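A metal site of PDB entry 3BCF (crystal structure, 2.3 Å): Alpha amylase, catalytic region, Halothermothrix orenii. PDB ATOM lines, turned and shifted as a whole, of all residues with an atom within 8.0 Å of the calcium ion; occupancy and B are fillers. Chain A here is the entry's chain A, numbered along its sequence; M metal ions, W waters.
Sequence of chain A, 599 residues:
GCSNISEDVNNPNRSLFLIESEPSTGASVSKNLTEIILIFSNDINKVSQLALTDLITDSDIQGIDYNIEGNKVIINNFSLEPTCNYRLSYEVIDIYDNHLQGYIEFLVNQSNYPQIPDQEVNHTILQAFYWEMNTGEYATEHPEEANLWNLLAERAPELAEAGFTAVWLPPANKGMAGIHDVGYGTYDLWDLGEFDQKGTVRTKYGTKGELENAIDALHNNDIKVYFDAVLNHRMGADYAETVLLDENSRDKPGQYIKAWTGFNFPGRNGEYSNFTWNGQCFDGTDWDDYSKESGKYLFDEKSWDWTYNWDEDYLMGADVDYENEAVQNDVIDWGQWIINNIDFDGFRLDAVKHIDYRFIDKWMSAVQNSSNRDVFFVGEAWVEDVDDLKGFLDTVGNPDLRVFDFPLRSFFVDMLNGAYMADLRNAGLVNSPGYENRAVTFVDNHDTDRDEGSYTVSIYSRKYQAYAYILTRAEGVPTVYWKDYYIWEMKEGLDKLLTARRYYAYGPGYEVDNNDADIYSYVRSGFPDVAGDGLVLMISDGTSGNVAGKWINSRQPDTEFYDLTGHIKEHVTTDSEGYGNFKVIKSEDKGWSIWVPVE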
ATOM      1  N   PRO A 114      -8.767  23.966 -18.798  1.00  0.00           N
ATOM      2  CA  PRO A 114      -9.218  22.602 -18.543  1.00  0.00           C
ATOM      3  C   PRO A 114     -10.599  22.539 -17.920  1.00  0.00           C
ATOM      4  O   PRO A 114     -10.984  23.400 -17.084  1.00  0.00           O
ATOM      5  CB  PRO A 114      -8.178  22.074 -17.582  1.00  0.00           C
ATOM      6  CG  PRO A 114      -6.991  22.887 -17.832  1.00  0.00           C
ATOM      7  CD  PRO A 114      -7.463  24.219 -18.189  1.00  0.00           C
ATOM      8  N   ILE A 116     -13.114  21.023 -15.577  1.00  0.00           N
ATOM      9  CA  ILE A 116     -13.166  20.238 -14.357  1.00  0.00           C
ATOM     10  C   ILE A 116     -14.614  19.960 -13.955  1.00  0.00           C
ATOM     11  O   ILE A 116     -15.388  20.893 -13.763  1.00  0.00           O
ATOM     12  CB  ILE A 116     -12.459  20.976 -13.148  1.00  0.00           C
ATOM     13  CG1 ILE A 116     -11.047  21.492 -13.485  1.00  0.00           C
ATOM     14  CG2 ILE A 116     -12.352  20.061 -11.973  1.00  0.00           C
ATOM     15  CD1 ILE A 116     -10.081  20.460 -13.983  1.00  0.00           C
ATOM     16  N   TYR A 504      -5.962  23.631 -12.528  1.00  0.00           N
ATOM     17  CA  TYR A 504      -4.821  22.759 -12.771  1.00  0.00           C
ATOM     18  C   TYR A 504      -4.442  21.798 -11.662  1.00  0.00           C
ATOM     19  O   TYR A 504      -3.949  20.687 -11.962  1.00  0.00           O
ATOM     20  CB  TYR A 504      -3.600  23.607 -13.170  1.00  0.00           C
ATOM     21  CG  TYR A 504      -3.808  24.420 -14.468  1.00  0.00           C
ATOM     22  CD1 TYR A 504      -4.183  25.740 -14.396  1.00  0.00           C
ATOM     23  CD2 TYR A 504      -3.675  23.848 -15.716  1.00  0.00           C
ATOM     24  CE1 TYR A 504      -4.377  26.474 -15.521  1.00  0.00           C
ATOM     25  CE2 TYR A 504      -3.867  24.581 -16.858  1.00  0.00           C
ATOM     26  CZ  TYR A 504      -4.220  25.904 -16.747  1.00  0.00           C
ATOM     27  OH  TYR A 504      -4.452  26.748 -17.827  1.00  0.00           O
ATOM     28  N   TYR A 506      -4.921  19.254  -9.738  1.00  0.00           N
ATOM     29  CA  TYR A 506      -5.929  18.201  -9.757  1.00  0.00           C
ATOM     30  C   TYR A 506      -5.195  16.899  -9.908  1.00  0.00           C
ATOM     31  O   TYR A 506      -4.109  16.901 -10.485  1.00  0.00           O
ATOM     32  CB  TYR A 506      -6.971  18.460 -10.895  1.00  0.00           C
ATOM     33  CG  TYR A 506      -7.931  19.574 -10.513  1.00  0.00           C
ATOM     34  CD1 TYR A 506      -7.786  20.836 -11.026  1.00  0.00           C
ATOM     35  CD2 TYR A 506      -8.924  19.384  -9.566  1.00  0.00           C
ATOM     36  CE1 TYR A 506      -8.580  21.840 -10.684  1.00  0.00           C
ATOM     37  CE2 TYR A 506      -9.744  20.428  -9.195  1.00  0.00           C
ATOM     38  CZ  TYR A 506      -9.561  21.653  -9.758  1.00  0.00           C
ATOM     39  OH  TYR A 506     -10.335  22.727  -9.411  1.00  0.00           O
ATOM     40  N   GLY A 507      -5.741  15.823  -9.332  1.00  0.00           N
ATOM     41  CA  GLY A 507      -5.151  14.457  -9.480  1.00  0.00           C
ATOM     42  C   GLY A 507      -4.186  14.169  -8.348  1.00  0.00           C
ATOM     43  O   GLY A 507      -3.970  15.029  -7.493  1.00  0.00           O
ATOM     44  N   ARG A 524       1.454  17.734  -9.330  1.00  0.00           N
ATOM     45  CA  ARG A 524       0.050  17.310  -9.456  1.00  0.00           C
ATOM     46  C   ARG A 524      -0.057  16.848 -10.895  1.00  0.00           C
ATOM     47  O   ARG A 524       0.156  17.669 -11.813  1.00  0.00           O
ATOM     48  CB  ARG A 524      -0.934  18.486  -9.300  1.00  0.00           C
ATOM     49  CG  ARG A 524      -0.955  19.203  -7.960  1.00  0.00           C
ATOM     50  CD  ARG A 524      -1.288  18.313  -6.812  1.00  0.00           C
ATOM     51  NE  ARG A 524      -2.581  17.669  -6.904  1.00  0.00           N
ATOM     52  CZ  ARG A 524      -3.704  18.190  -6.422  1.00  0.00           C
ATOM     53  NH1 ARG A 524      -3.713  19.374  -5.859  1.00  0.00           N
ATOM     54  NH2 ARG A 524      -4.820  17.534  -6.499  1.00  0.00           N
ATOM     55  N   SER A 525      -0.400  15.592 -11.093  1.00  0.00           N
ATOM     56  CA  SER A 525      -0.343  14.927 -12.395  1.00  0.00           C
ATOM     57  C   SER A 525      -1.548  15.220 -13.270  1.00  0.00           C
ATOM     58  O   SER A 525      -1.533  14.875 -14.431  1.00  0.00           O
ATOM     59  CB  SER A 525      -0.260  13.407 -12.229  1.00  0.00           C
ATOM     60  OG  SER A 525      -1.481  12.915 -11.719  1.00  0.00           O
ATOM     61  N   GLY A 526      -2.586  15.843 -12.710  1.00  0.00           N
ATOM     62  CA  GLY A 526      -3.816  16.058 -13.478  1.00  0.00           C
ATOM     63  C   GLY A 526      -4.709  14.847 -13.407  1.00  0.00           C
ATOM     64  O   GLY A 526      -4.265  13.780 -12.949  1.00  0.00           O
ATOM     65  N   PHE A 527      -5.972  14.987 -13.823  1.00  0.00           N
ATOM     66  CA  PHE A 527      -6.879  13.830 -13.923  1.00  0.00           C
ATOM     67  C   PHE A 527      -6.634  13.157 -15.273  1.00  0.00           C
ATOM     68  O   PHE A 527      -6.445  13.823 -16.290  1.00  0.00           O
ATOM     69  CB  PHE A 527      -8.368  14.198 -13.842  1.00  0.00           C
ATOM     70  CG  PHE A 527      -8.845  14.571 -12.466  1.00  0.00           C
ATOM     71  CD1 PHE A 527      -9.453  15.791 -12.252  1.00  0.00           C
ATOM     72  CD2 PHE A 527      -8.681  13.710 -11.408  1.00  0.00           C
ATOM     73  CE1 PHE A 527      -9.896  16.151 -11.021  1.00  0.00           C
ATOM     74  CE2 PHE A 527      -9.113  14.062 -10.163  1.00  0.00           C
ATOM     75  CZ  PHE A 527      -9.732  15.289  -9.963  1.00  0.00           C
ATOM     76  N   PRO A 528      -6.677  11.830 -15.295  1.00  0.00           N
ATOM     77  CA  PRO A 528      -6.490  11.121 -16.559  1.00  0.00           C
ATOM     78  C   PRO A 528      -7.613  11.460 -17.535  1.00  0.00           C
ATOM     79  O   PRO A 528      -7.333  11.770 -18.682  1.00  0.00           O
ATOM     80  CB  PRO A 528      -6.544   9.639 -16.150  1.00  0.00           C
ATOM     81  CG  PRO A 528      -6.407   9.601 -14.654  1.00  0.00           C
ATOM     82  CD  PRO A 528      -6.901  10.918 -14.150  1.00  0.00           C
ATOM     83  N   ASP A 529      -8.847  11.441 -17.053  1.00  0.00           N
ATOM     84  CA  ASP A 529     -10.032  11.754 -17.879  1.00  0.00           C
ATOM     85  C   ASP A 529     -10.316  13.300 -18.088  1.00  0.00           C
ATOM     86  O   ASP A 529     -11.394  13.687 -18.589  1.00  0.00           O
ATOM     87  CB  ASP A 529     -11.273  11.035 -17.327  1.00  0.00           C
ATOM     88  CG  ASP A 529     -11.563  11.355 -15.826  1.00  0.00           C
ATOM     89  OD1 ASP A 529     -11.000  12.308 -15.197  1.00  0.00           O
ATOM     90  OD2 ASP A 529     -12.417  10.619 -15.269  1.00  0.00           O
ATOM     91  N   VAL A 530      -9.351  14.146 -17.734  1.00  0.00           N
ATOM     92  CA  VAL A 530      -9.413  15.553 -18.059  1.00  0.00           C
ATOM     93  C   VAL A 530      -8.172  15.986 -18.838  1.00  0.00           C
ATOM     94  O   VAL A 530      -7.057  15.694 -18.431  1.00  0.00           O
ATOM     95  CB  VAL A 530      -9.524  16.413 -16.780  1.00  0.00           C
ATOM     96  CG1 VAL A 530      -9.593  17.890 -17.146  1.00  0.00           C
ATOM     97  CG2 VAL A 530     -10.739  15.972 -15.943  1.00  0.00           C
ATOM     98  N   ALA A 531      -8.379  16.702 -19.935  1.00  0.00           N
ATOM     99  CA  ALA A 531      -7.290  17.223 -20.752  1.00  0.00           C
ATOM    100  C   ALA A 531      -6.707  18.560 -20.253  1.00  0.00           C
ATOM    101  O   ALA A 531      -7.432  19.526 -19.931  1.00  0.00           O
ATOM    102  CB  ALA A 531      -7.723  17.364 -22.203  1.00  0.00           C
ATOM    103  N   GLY A 532      -5.383  18.592 -20.190  1.00  0.00           N
ATOM    104  CA  GLY A 532      -4.644  19.825 -19.996  1.00  0.00           C
ATOM    105  C   GLY A 532      -4.570  20.339 -18.573  1.00  0.00           C
ATOM    106  O   GLY A 532      -4.099  21.464 -18.366  1.00  0.00           O
ATOM    107  N   ASP A 533      -5.017  19.536 -17.592  1.00  0.00           N
ATOM    108  CA  ASP A 533      -4.810  19.900 -16.187  1.00  0.00           C
ATOM    109  C   ASP A 533      -3.452  19.352 -15.679  1.00  0.00           C
ATOM    110  O   ASP A 533      -2.634  18.862 -16.464  1.00  0.00           O
ATOM    111  CB  ASP A 533      -6.005  19.503 -15.303  1.00  0.00           C
ATOM    112  CG  ASP A 533      -6.114  18.011 -15.102  1.00  0.00           C
ATOM    113  OD1 ASP A 533      -5.555  17.286 -15.917  1.00  0.00           O
ATOM    114  OD2 ASP A 533      -6.782  17.563 -14.150  1.00  0.00           O
ATOM    115  N   GLY A 534      -3.181  19.505 -14.378  1.00  0.00           N
ATOM    116  CA  GLY A 534      -1.849  19.108 -13.814  1.00  0.00           C
ATOM    117  C   GLY A 534      -0.844  20.267 -13.738  1.00  0.00           C
ATOM    118  O   GLY A 534      -1.013  21.321 -14.375  1.00  0.00           O
ATOM    119  N   ARG A 555       4.756  13.322 -14.999  1.00  0.00           N
ATOM    120  CA  ARG A 555       3.698  12.327 -15.184  1.00  0.00           C
ATOM    121  C   ARG A 555       2.847  12.651 -16.433  1.00  0.00           C
ATOM    122  O   ARG A 555       1.732  12.143 -16.561  1.00  0.00           O
ATOM    123  CB  ARG A 555       2.742  12.271 -13.963  1.00  0.00           C
ATOM    124  CG  ARG A 555       3.141  11.378 -12.808  1.00  0.00           C
ATOM    125  CD  ARG A 555       4.454  11.778 -12.132  1.00  0.00           C
ATOM    126  NE  ARG A 555       4.850  10.723 -11.195  1.00  0.00           N
ATOM    127  CZ  ARG A 555       5.824  10.822 -10.294  1.00  0.00           C
ATOM    128  NH1 ARG A 555       6.552  11.926 -10.199  1.00  0.00           N
ATOM    129  NH2 ARG A 555       6.068   9.800  -9.481  1.00  0.00           N
ATOM    130  N   GLN A 556       3.342  13.497 -17.320  1.00  0.00           N
ATOM    131  CA  GLN A 556       2.634  13.788 -18.564  1.00  0.00           C
ATOM    132  C   GLN A 556       3.665  13.732 -19.682  1.00  0.00           C
ATOM    133  O   GLN A 556       4.348  14.712 -19.975  1.00  0.00           O
ATOM    134  CB  GLN A 556       1.934  15.139 -18.529  1.00  0.00           C
ATOM    135  CG  GLN A 556       0.959  15.341 -17.370  1.00  0.00           C
ATOM    136  CD  GLN A 556       0.104  16.591 -17.508  1.00  0.00           C
ATOM    137  OE1 GLN A 556      -0.655  16.746 -18.459  1.00  0.00           O
ATOM    138  NE2 GLN A 556       0.215  17.482 -16.550  1.00  0.00           N
ATOM    139  N   PRO A 597       0.302  22.929 -18.466  1.00  0.00           N
ATOM    140  CA  PRO A 597       0.323  22.696 -19.910  1.00  0.00           C
ATOM    141  C   PRO A 597      -0.159  23.927 -20.726  1.00  0.00           C
ATOM    142  O   PRO A 597      -0.998  24.724 -20.243  1.00  0.00           O
ATOM    143  CB  PRO A 597      -0.593  21.481 -20.072  1.00  0.00           C
ATOM    144  CG  PRO A 597      -0.760  20.911 -18.663  1.00  0.00           C
ATOM    145  CD  PRO A 597      -0.662  22.072 -17.767  1.00  0.00           C
HETATM  146 CA    CA M   1      -5.056  15.447 -17.189  1.00  0.00          CA
HETATM  147  O   HOH W   1      -3.345  16.731 -18.066  1.00  0.00           O
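NE2 of Gln 556 is in hydrogen-bond range of O of Asp 533 (3.2 Å). The backbone NH (N) of Gly 526 is in hydrogen-bond range of the backbone carbonyl oxygen (O) of Tyr 506 (2.9 Å).
Residues that only touch the calcium ion: Gly 526 (3.8 Å). Of the 19 residues printed, 4 come within 4 Å of the calcium ion. The nearest printed residue that does not touch the calcium ion is Gly 532 (4.4 Å).
The calcium ion is bound by OD1 of Asp 533 (2.3 Å), water W1 (2.3 Å), O of Phe 527 (2.3 Å) and O of Val 530 (2.4 Å). The calcium ion has four donor atoms within binding distance.
Water W1 lies within hydrogen-bond range of the side-chain amide oxygen of Gln 556, the backbone carbonyl oxygen of Asp 533 and the backbone NH of Gly 532.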
